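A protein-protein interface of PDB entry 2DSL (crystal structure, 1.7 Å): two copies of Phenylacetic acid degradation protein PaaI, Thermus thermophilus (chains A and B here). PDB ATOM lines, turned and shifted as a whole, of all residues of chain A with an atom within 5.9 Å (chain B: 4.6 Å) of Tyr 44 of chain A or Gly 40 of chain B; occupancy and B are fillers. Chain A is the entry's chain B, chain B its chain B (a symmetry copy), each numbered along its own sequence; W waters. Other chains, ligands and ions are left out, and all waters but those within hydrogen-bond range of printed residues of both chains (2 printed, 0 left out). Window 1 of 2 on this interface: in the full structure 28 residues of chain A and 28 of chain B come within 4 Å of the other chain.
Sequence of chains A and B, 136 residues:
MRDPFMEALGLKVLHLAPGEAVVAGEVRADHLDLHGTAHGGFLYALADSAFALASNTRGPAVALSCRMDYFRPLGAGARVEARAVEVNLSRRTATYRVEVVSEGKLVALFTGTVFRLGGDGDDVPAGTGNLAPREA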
ATOM      1  N   PHE A   5       7.470  -3.977  -8.926  1.00  0.00           N
ATOM      2  CA  PHE A   5       8.080  -4.599 -10.095  1.00  0.00           C
ATOM      3  C   PHE A   5       9.435  -3.966 -10.397  1.00  0.00           C
ATOM      4  O   PHE A   5      10.387  -4.661 -10.742  1.00  0.00           O
ATOM      5  CB  PHE A   5       7.148  -4.487 -11.311  1.00  0.00           C
ATOM      6  CG  PHE A   5       7.517  -5.405 -12.446  1.00  0.00           C
ATOM      7  CD1 PHE A   5       7.745  -6.759 -12.216  1.00  0.00           C
ATOM      8  CD2 PHE A   5       7.617  -4.920 -13.748  1.00  0.00           C
ATOM      9  CE1 PHE A   5       8.067  -7.619 -13.269  1.00  0.00           C
ATOM     10  CE2 PHE A   5       7.935  -5.768 -14.805  1.00  0.00           C
ATOM     11  CZ  PHE A   5       8.161  -7.119 -14.567  1.00  0.00           C
ATOM     12  N   HIS A  39      15.884 -10.222 -22.235  1.00  0.00           N
ATOM     13  CA  HIS A  39      14.514 -10.480 -22.670  1.00  0.00           C
ATOM     14  C   HIS A  39      13.825  -9.170 -23.056  1.00  0.00           C
ATOM     15  O   HIS A  39      14.024  -8.129 -22.445  1.00  0.00           O
ATOM     16  CB  HIS A  39      13.776 -11.135 -21.481  1.00  0.00           C
ATOM     17  CG  HIS A  39      12.452 -11.742 -21.901  1.00  0.00           C
ATOM     18  ND1 HIS A  39      11.355 -11.003 -22.227  1.00  0.00           N
ATOM     19  CD2 HIS A  39      12.091 -13.101 -21.954  1.00  0.00           C
ATOM     20  CE1 HIS A  39      10.378 -11.894 -22.487  1.00  0.00           C
ATOM     21  NE2 HIS A  39      10.788 -13.157 -22.332  1.00  0.00           N
ATOM     22  N   GLY A  40      13.033  -9.242 -24.138  1.00  0.00           N
ATOM     23  CA  GLY A  40      12.334  -8.048 -24.606  1.00  0.00           C
ATOM     24  C   GLY A  40      11.475  -7.426 -23.505  1.00  0.00           C
ATOM     25  O   GLY A  40      11.234  -6.229 -23.473  1.00  0.00           O
ATOM     26  N   GLY A  41      10.975  -8.300 -22.607  1.00  0.00           N
ATOM     27  CA  GLY A  41      10.113  -7.828 -21.529  1.00  0.00           C
ATOM     28  C   GLY A  41      10.887  -7.035 -20.476  1.00  0.00           C
ATOM     29  O   GLY A  41      10.348  -6.169 -19.798  1.00  0.00           O
ATOM     30  N   PHE A  42      12.184  -7.389 -20.305  1.00  0.00           N
ATOM     31  CA  PHE A  42      12.996  -6.663 -19.330  1.00  0.00           C
ATOM     32  C   PHE A  42      13.291  -5.256 -19.827  1.00  0.00           C
ATOM     33  O   PHE A  42      13.154  -4.280 -19.110  1.00  0.00           O
ATOM     34  CB  PHE A  42      14.308  -7.435 -19.086  1.00  0.00           C
ATOM     35  CG  PHE A  42      15.251  -6.645 -18.203  1.00  0.00           C
ATOM     36  CD1 PHE A  42      14.947  -6.441 -16.854  1.00  0.00           C
ATOM     37  CD2 PHE A  42      16.409  -6.092 -18.738  1.00  0.00           C
ATOM     38  CE1 PHE A  42      15.788  -5.667 -16.065  1.00  0.00           C
ATOM     39  CE2 PHE A  42      17.244  -5.318 -17.935  1.00  0.00           C
ATOM     40  CZ  PHE A  42      16.938  -5.099 -16.598  1.00  0.00           C
ATOM     41  N   LEU A  43      13.745  -5.184 -21.098  1.00  0.00           N
ATOM     42  CA  LEU A  43      14.052  -3.871 -21.660  1.00  0.00           C
ATOM     43  C   LEU A  43      12.803  -2.994 -21.704  1.00  0.00           C
ATOM     44  O   LEU A  43      12.849  -1.794 -21.477  1.00  0.00           O
ATOM     45  CB  LEU A  43      14.632  -4.048 -23.063  1.00  0.00           C
ATOM     46  CG  LEU A  43      15.994  -4.716 -23.048  1.00  0.00           C
ATOM     47  CD1 LEU A  43      16.560  -4.879 -24.472  1.00  0.00           C
ATOM     48  CD2 LEU A  43      17.017  -3.913 -22.237  1.00  0.00           C
ATOM     49  N   TYR A  44      11.655  -3.627 -22.034  1.00  0.00           N
ATOM     50  CA  TYR A  44      10.409  -2.859 -22.056  1.00  0.00           C
ATOM     51  C   TYR A  44      10.042  -2.403 -20.649  1.00  0.00           C
ATOM     52  O   TYR A  44       9.626  -1.278 -20.433  1.00  0.00           O
ATOM     53  CB  TYR A  44       9.281  -3.722 -22.667  1.00  0.00           C
ATOM     54  CG  TYR A  44       7.958  -2.998 -22.695  1.00  0.00           C
ATOM     55  CD1 TYR A  44       7.136  -2.975 -21.559  1.00  0.00           C
ATOM     56  CD2 TYR A  44       7.490  -2.409 -23.876  1.00  0.00           C
ATOM     57  CE1 TYR A  44       5.890  -2.348 -21.602  1.00  0.00           C
ATOM     58  CE2 TYR A  44       6.246  -1.788 -23.913  1.00  0.00           C
ATOM     59  CZ  TYR A  44       5.446  -1.761 -22.788  1.00  0.00           C
ATOM     60  OH  TYR A  44       4.200  -1.159 -22.832  1.00  0.00           O
ATOM     61  N   ALA A  45      10.185  -3.332 -19.676  1.00  0.00           N
ATOM     62  CA  ALA A  45       9.854  -2.963 -18.299  1.00  0.00           C
ATOM     63  C   ALA A  45      10.666  -1.752 -17.853  1.00  0.00           C
ATOM     64  O   ALA A  45      10.181  -0.871 -17.154  1.00  0.00           O
ATOM     65  CB  ALA A  45      10.126  -4.156 -17.380  1.00  0.00           C
ATOM     66  N   LEU A  46      11.955  -1.743 -18.263  1.00  0.00           N
ATOM     67  CA  LEU A  46      12.830  -0.620 -17.915  1.00  0.00           C
ATOM     68  C   LEU A  46      12.293   0.689 -18.483  1.00  0.00           C
ATOM     69  O   LEU A  46      12.123   1.675 -17.782  1.00  0.00           O
ATOM     70  CB  LEU A  46      14.220  -0.914 -18.479  1.00  0.00           C
ATOM     71  CG  LEU A  46      15.181   0.259 -18.378  1.00  0.00           C
ATOM     72  CD1 LEU A  46      15.708   0.443 -16.943  1.00  0.00           C
ATOM     73  CD2 LEU A  46      16.409   0.058 -19.281  1.00  0.00           C
ATOM     74  N   ALA A  47      12.056   0.677 -19.813  1.00  0.00           N
ATOM     75  CA  ALA A  47      11.557   1.881 -20.475  1.00  0.00           C
ATOM     76  C   ALA A  47      10.199   2.306 -19.922  1.00  0.00           C
ATOM     77  O   ALA A  47       9.932   3.479 -19.689  1.00  0.00           O
ATOM     78  CB  ALA A  47      11.453   1.602 -21.977  1.00  0.00           C
ATOM     79  N   ASP A  48       9.316   1.302 -19.746  1.00  0.00           N
ATOM     80  CA  ASP A  48       7.976   1.580 -19.229  1.00  0.00           C
ATOM     81  C   ASP A  48       8.023   2.219 -17.840  1.00  0.00           C
ATOM     82  O   ASP A  48       7.191   3.038 -17.489  1.00  0.00           O
ATOM     83  CB  ASP A  48       7.198   0.258 -19.195  1.00  0.00           C
ATOM     84  CG  ASP A  48       5.754   0.494 -18.754  1.00  0.00           C
ATOM     85  OD1 ASP A  48       5.018   1.155 -19.496  1.00  0.00           O
ATOM     86  OD2 ASP A  48       5.374  -0.011 -17.698  1.00  0.00           O
ATOM     87  N   SER A  49       9.014   1.786 -17.027  1.00  0.00           N
ATOM     88  CA  SER A  49       9.114   2.359 -15.684  1.00  0.00           C
ATOM     89  C   SER A  49       9.470   3.844 -15.740  1.00  0.00           C
ATOM     90  O   SER A  49       8.965   4.655 -14.976  1.00  0.00           O
ATOM     91  CB  SER A  49      10.161   1.589 -14.874  1.00  0.00           C
ATOM     92  OG  SER A  49       9.688   0.260 -14.616  1.00  0.00           O
ATOM     93  N   CYS A  66       1.667   1.657 -26.083  1.00  0.00           N
ATOM     94  CA  CYS A  66       3.116   1.812 -26.116  1.00  0.00           C
ATOM     95  C   CYS A  66       3.726   0.995 -27.241  1.00  0.00           C
ATOM     96  O   CYS A  66       3.226  -0.058 -27.626  1.00  0.00           O
ATOM     97  CB  CYS A  66       3.701   1.301 -24.794  1.00  0.00           C
ATOM     98  SG  CYS A  66       2.977   2.095 -23.340  1.00  0.00           S
ATOM     99  N   ARG A  67       4.824   1.541 -27.803  1.00  0.00           N
ATOM    100  CA  ARG A  67       5.574   0.851 -28.850  1.00  0.00           C
ATOM    101  C   ARG A  67       7.019   0.705 -28.421  1.00  0.00           C
ATOM    102  O   ARG A  67       7.588   1.566 -27.761  1.00  0.00           O
ATOM    103  CB  ARG A  67       5.524   1.701 -30.132  1.00  0.00           C
ATOM    104  CG  ARG A  67       6.411   1.164 -31.271  1.00  0.00           C
ATOM    105  CD  ARG A  67       6.292   2.054 -32.530  1.00  0.00           C
ATOM    106  NE  ARG A  67       7.274   1.678 -33.560  1.00  0.00           N
ATOM    107  CZ  ARG A  67       6.855   1.150 -34.742  1.00  0.00           C
ATOM    108  NH1 ARG A  67       5.566   0.932 -34.992  1.00  0.00           N
ATOM    109  NH2 ARG A  67       7.766   0.860 -35.667  1.00  0.00           N
ATOM    110  N   MET A  68       7.597  -0.455 -28.763  1.00  0.00           N
ATOM    111  CA  MET A  68       8.990  -0.704 -28.440  1.00  0.00           C
ATOM    112  C   MET A  68       9.728  -1.210 -29.669  1.00  0.00           C
ATOM    113  O   MET A  68       9.336  -2.185 -30.301  1.00  0.00           O
ATOM    114  CB  MET A  68       9.036  -1.769 -27.338  1.00  0.00           C
ATOM    115  CG  MET A  68      10.475  -2.107 -26.908  1.00  0.00           C
ATOM    116  SD  MET A  68      11.135  -0.817 -25.847  1.00  0.00           S
ATOM    117  CE  MET A  68      12.466  -1.775 -25.085  1.00  0.00           C
ATOM    118  N   TYR A  70      13.378  -2.488 -31.022  1.00  0.00           N
ATOM    119  CA  TYR A  70      14.653  -3.045 -30.566  1.00  0.00           C
ATOM    120  C   TYR A  70      15.728  -2.948 -31.657  1.00  0.00           C
ATOM    121  O   TYR A  70      15.506  -3.281 -32.817  1.00  0.00           O
ATOM    122  CB  TYR A  70      14.432  -4.541 -30.247  1.00  0.00           C
ATOM    123  CG  TYR A  70      13.419  -4.743 -29.159  1.00  0.00           C
ATOM    124  CD1 TYR A  70      13.817  -4.741 -27.819  1.00  0.00           C
ATOM    125  CD2 TYR A  70      12.079  -4.996 -29.470  1.00  0.00           C
ATOM    126  CE1 TYR A  70      12.884  -4.960 -26.808  1.00  0.00           C
ATOM    127  CE2 TYR A  70      11.153  -5.219 -28.457  1.00  0.00           C
ATOM    128  CZ  TYR A  70      11.551  -5.208 -27.133  1.00  0.00           C
ATOM    129  OH  TYR A  70      10.638  -5.458 -26.123  1.00  0.00           O
ATOM    130  N   PHE A 110      11.344   3.524 -27.142  1.00  0.00           N
ATOM    131  CA  PHE A 110      10.003   3.312 -26.614  1.00  0.00           C
ATOM    132  C   PHE A 110       9.174   4.581 -26.813  1.00  0.00           C
ATOM    133  O   PHE A 110       9.658   5.696 -26.612  1.00  0.00           O
ATOM    134  CB  PHE A 110      10.134   2.953 -25.122  1.00  0.00           C
ATOM    135  CG  PHE A 110       8.828   2.859 -24.366  1.00  0.00           C
ATOM    136  CD1 PHE A 110       8.111   4.006 -24.032  1.00  0.00           C
ATOM    137  CD2 PHE A 110       8.365   1.623 -23.911  1.00  0.00           C
ATOM    138  CE1 PHE A 110       6.955   3.926 -23.249  1.00  0.00           C
ATOM    139  CE2 PHE A 110       7.209   1.532 -23.125  1.00  0.00           C
ATOM    140  CZ  PHE A 110       6.507   2.687 -22.795  1.00  0.00           C
ATOM    141  N   ALA B  38      -1.218  -4.382 -11.786  1.00  0.00           N
ATOM    142  CA  ALA B  38      -0.193  -5.038 -12.595  1.00  0.00           C
ATOM    143  C   ALA B  38       0.607  -4.045 -13.434  1.00  0.00           C
ATOM    144  O   ALA B  38       0.067  -3.249 -14.196  1.00  0.00           O
ATOM    145  CB  ALA B  38      -0.872  -6.054 -13.517  1.00  0.00           C
ATOM    146  N   HIS B  39       1.945  -4.093 -13.244  1.00  0.00           N
ATOM    147  CA  HIS B  39       2.848  -3.201 -13.966  1.00  0.00           C
ATOM    148  C   HIS B  39       2.773  -3.475 -15.469  1.00  0.00           C
ATOM    149  O   HIS B  39       2.640  -4.606 -15.915  1.00  0.00           O
ATOM    150  CB  HIS B  39       4.275  -3.482 -13.448  1.00  0.00           C
ATOM    151  CG  HIS B  39       5.256  -2.409 -13.877  1.00  0.00           C
ATOM    152  ND1 HIS B  39       5.705  -2.268 -15.156  1.00  0.00           N
ATOM    153  CD2 HIS B  39       5.918  -1.458 -13.078  1.00  0.00           C
ATOM    154  CE1 HIS B  39       6.589  -1.252 -15.124  1.00  0.00           C
ATOM    155  NE2 HIS B  39       6.738  -0.748 -13.895  1.00  0.00           N
ATOM    156  N   GLY B  40       2.813  -2.382 -16.249  1.00  0.00           N
ATOM    157  CA  GLY B  40       2.736  -2.525 -17.701  1.00  0.00           C
ATOM    158  C   GLY B  40       3.823  -3.456 -18.237  1.00  0.00           C
ATOM    159  O   GLY B  40       3.666  -4.113 -19.255  1.00  0.00           O
ATOM    160  N   GLY B  41       4.971  -3.462 -17.530  1.00  0.00           N
ATOM    161  CA  GLY B  41       6.094  -4.287 -17.964  1.00  0.00           C
ATOM    162  C   GLY B  41       5.833  -5.777 -17.745  1.00  0.00           C
ATOM    163  O   GLY B  41       6.365  -6.632 -18.443  1.00  0.00           O
ATOM    164  N   PHE B  42       5.028  -6.089 -16.701  1.00  0.00           N
ATOM    165  CA  PHE B  42       4.715  -7.493 -16.439  1.00  0.00           C
ATOM    166  C   PHE B  42       3.786  -8.040 -17.512  1.00  0.00           C
ATOM    167  O   PHE B  42       3.993  -9.110 -18.055  1.00  0.00           O
ATOM    168  CB  PHE B  42       4.065  -7.618 -15.047  1.00  0.00           C
ATOM    169  CG  PHE B  42       3.581  -9.030 -14.794  1.00  0.00           C
ATOM    170  CD1 PHE B  42       4.499 -10.068 -14.620  1.00  0.00           C
ATOM    171  CD2 PHE B  42       2.218  -9.305 -14.765  1.00  0.00           C
ATOM    172  CE1 PHE B  42       4.048 -11.369 -14.447  1.00  0.00           C
ATOM    173  CE2 PHE B  42       1.779 -10.615 -14.589  1.00  0.00           C
ATOM    174  CZ  PHE B  42       2.688 -11.654 -14.432  1.00  0.00           C
ATOM    175  N   LEU B  43       2.710  -7.268 -17.781  1.00  0.00           N
ATOM    176  CA  LEU B  43       1.764  -7.713 -18.801  1.00  0.00           C
ATOM    177  C   LEU B  43       2.444  -7.820 -20.163  1.00  0.00           C
ATOM    178  O   LEU B  43       2.171  -8.711 -20.953  1.00  0.00           O
ATOM    179  CB  LEU B  43       0.593  -6.734 -18.862  1.00  0.00           C
ATOM    180  CG  LEU B  43      -0.255  -6.763 -17.605  1.00  0.00           C
ATOM    181  CD1 LEU B  43      -1.433  -5.772 -17.692  1.00  0.00           C
ATOM    182  CD2 LEU B  43      -0.845  -8.154 -17.343  1.00  0.00           C
ATOM    183  N   TYR B  44       3.346  -6.851 -20.444  1.00  0.00           N
ATOM    184  CA  TYR B  44       4.070  -6.911 -21.715  1.00  0.00           C
ATOM    185  C   TYR B  44       4.993  -8.123 -21.744  1.00  0.00           C
ATOM    186  O   TYR B  44       5.095  -8.821 -22.736  1.00  0.00           O
ATOM    187  CB  TYR B  44       4.869  -5.603 -21.915  1.00  0.00           C
ATOM    188  CG  TYR B  44       5.663  -5.609 -23.198  1.00  0.00           C
ATOM    189  CD1 TYR B  44       6.922  -6.224 -23.253  1.00  0.00           C
ATOM    190  CD2 TYR B  44       5.196  -4.930 -24.331  1.00  0.00           C
ATOM    191  CE1 TYR B  44       7.676  -6.185 -24.427  1.00  0.00           C
ATOM    192  CE2 TYR B  44       5.954  -4.892 -25.495  1.00  0.00           C
ATOM    193  CZ  TYR B  44       7.189  -5.508 -25.546  1.00  0.00           C
ATOM    194  OH  TYR B  44       7.950  -5.454 -26.701  1.00  0.00           O
ATOM    195  N   MET B  68       1.824  -2.455 -27.526  1.00  0.00           N
ATOM    196  CA  MET B  68       0.994  -2.972 -26.452  1.00  0.00           C
ATOM    197  C   MET B  68      -0.104  -1.976 -26.116  1.00  0.00           C
ATOM    198  O   MET B  68       0.147  -0.809 -25.834  1.00  0.00           O
ATOM    199  CB  MET B  68       1.890  -3.182 -25.225  1.00  0.00           C
ATOM    200  CG  MET B  68       1.111  -3.741 -24.020  1.00  0.00           C
ATOM    201  SD  MET B  68       0.795  -5.496 -24.233  1.00  0.00           S
ATOM    202  CE  MET B  68       0.471  -5.904 -22.501  1.00  0.00           C
ATOM    203  N   TYR B  70      -3.300  -1.313 -23.640  1.00  0.00           N
ATOM    204  CA  TYR B  70      -3.870  -1.712 -22.352  1.00  0.00           C
ATOM    205  C   TYR B  70      -5.337  -1.278 -22.230  1.00  0.00           C
ATOM    206  O   TYR B  70      -5.705  -0.145 -22.529  1.00  0.00           O
ATOM    207  CB  TYR B  70      -3.070  -1.003 -21.236  1.00  0.00           C
ATOM    208  CG  TYR B  70      -1.621  -1.391 -21.246  1.00  0.00           C
ATOM    209  CD1 TYR B  70      -1.191  -2.517 -20.536  1.00  0.00           C
ATOM    210  CD2 TYR B  70      -0.675  -0.604 -21.909  1.00  0.00           C
ATOM    211  CE1 TYR B  70       0.158  -2.863 -20.517  1.00  0.00           C
ATOM    212  CE2 TYR B  70       0.671  -0.951 -21.882  1.00  0.00           C
ATOM    213  CZ  TYR B  70       1.090  -2.069 -21.186  1.00  0.00           C
ATOM    214  OH  TYR B  70       2.433  -2.402 -21.133  1.00  0.00           O
HETATM  215  O   HOH W   1       2.577   0.518 -19.554  1.00  0.00           O
HETATM  216  O   HOH W   2       3.360   0.445 -15.962  1.00  0.00           O
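OH of Tyr 44 of chain A is in hydrogen-bond range of OH of Tyr 70 of chain B.
OD2 of Asp 48 of chain A sits close to ND1 of His 39 of chain B (3.4 Å).
N of Gly 41 of chain B sits at hydrogen-bond distance from OD2 of Asp 48 of chain A (3.5 Å).
OG of Ser 49 of chain A is in hydrogen-bond range of NE2 of His 39 of chain B, 3.2 Å away.
The backbone carbonyl oxygen of Cys 66 of chain A sits at hydrogen-bond distance from the backbone NH of Met 68 of chain B (2.8 Å).
The side-chain hydroxyl of Tyr 44 of chain B lies within hydrogen-bond range of the side-chain hydroxyl of Tyr 70 of chain A, 2.7 Å away.
The backbone NH of Gly 41 of chain A is in hydrogen-bond range of a ring nitrogen (ND1) of His 39 of chain A, 2.8 Å away.
OH of Tyr 70 of chain A is in hydrogen-bond range of O of Gly 40 of chain A (2.8 Å).
The side-chain hydroxyl (OH) of Tyr 44 of chain A sits close to the side-chain sulfur (SG) of Cys 66 of chain A (3.5 Å).
The backbone carbonyl oxygen (O) of Ala 45 of chain A sits at hydrogen-bond distance from the side-chain hydroxyl (OG) of Ser 49 of chain A.
A ring nitrogen (ND1) of His 39 of chain B sits at hydrogen-bond distance from the backbone NH (N) of Gly 41 of chain B, 2.8 Å away.
The backbone carbonyl oxygen (O) of Gly 40 of chain B sits at hydrogen-bond distance from the side-chain hydroxyl (OH) of Tyr 70 of chain B, at 2.8 Å.
Among the printed residues, merely in contact across the chains: Tyr 44 of chain A with Tyr 44 of chain B, Phe 5 of chain A with His 39 of chain B, Phe 5 of chain A with Phe 42 of chain B, Phe 5 of chain A with Gly 41 of chain B, Asp 48 of chain A with Gly 40 of chain B, Tyr 44 of chain A with Gly 40 of chain B, Gly 40 of chain A with Tyr 44 of chain B, Tyr 44 of chain A with Met 68 of chain B, Met 68 of chain A with Tyr 44 of chain B, Gly 41 of chain A with Tyr 44 of chain B and Tyr 44 of chain A with Gly 41 of chain B.
Of chain B, only Gly 40 (3.7 Å), Gly 41 (3.97 Å), Tyr 44 (3.3 Å), Met 68 (3.9 Å) and Tyr 70 (2.7 Å) come within 4 Å of Tyr 44 of chain A.
Printed residues of chain B within 4 Å of Met 68 of chain A: Tyr 44 (3.9 Å).
Printed residues of chain A within 4 Å of His 39 of chain B: Phe 5 (3.4 Å), Asp 48 (3.1 Å) and Ser 49 (3.2 Å).
Gly 40 of chain B touches two residues of chain A.
Of the printed residues of chain A, Gly 41 of chain B touches Phe 5 (3.6 Å), Tyr 44 (3.97 Å) and Asp 48 (3.5 Å).
Of the printed residues of chain A, Phe 42 of chain B touches Phe 5.
Of the printed residues of chain A, Tyr 70 of chain B touches Tyr 44.
The nearest residue of chain A that does not touch Gly 40 of chain B is Phe 5 of chain A (5.8 Å).
The nearest printed residue of chain B that does not touch Phe 5 of chain A is Gly 40 of chain B (5.8 Å).
Of the 9 printed residues of chain B, 7 touch a printed residue of chain A.
Of the 17 printed residues of chain A, 9 touch a printed residue of chain B.
Hydrophobic or aromatic side chains of chain A within 4 Å of the printed part of chain B: Phe 5, Tyr 44, Met 68 and Tyr 70.
Among the printed residues, 17 pairs touch across the chains.
Gly 40 of chain A touches Tyr 44 of chain B, and with the chains exchanged Tyr 44 of chain A touches Gly 40 of chain B.
Gly 41 of chain A touches Tyr 44 of chain B, and with the chains exchanged Tyr 44 of chain A touches Gly 41 of chain B.
Tyr 44 of chain A touches its own counterpart, Tyr 44 of chain B.
Tyr 44 of chain A touches Tyr 70 of chain B, and with the chains exchanged Tyr 70 of chain A touches Tyr 44 of chain B.
Of the 17 pairs that touch across the chains among the printed residues, 9 have their exchanged pair printed and touching as well.
Water W1 lies within hydrogen-bond range of the side-chain carboxylate of Asp 48 of chain A and the side-chain hydroxyl of Tyr 70 of chain B.
Water W2 bridges OD2 of Asp 48 of chain A (2.7 Å) and N of Gly 40 of chain B (2.9 Å).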
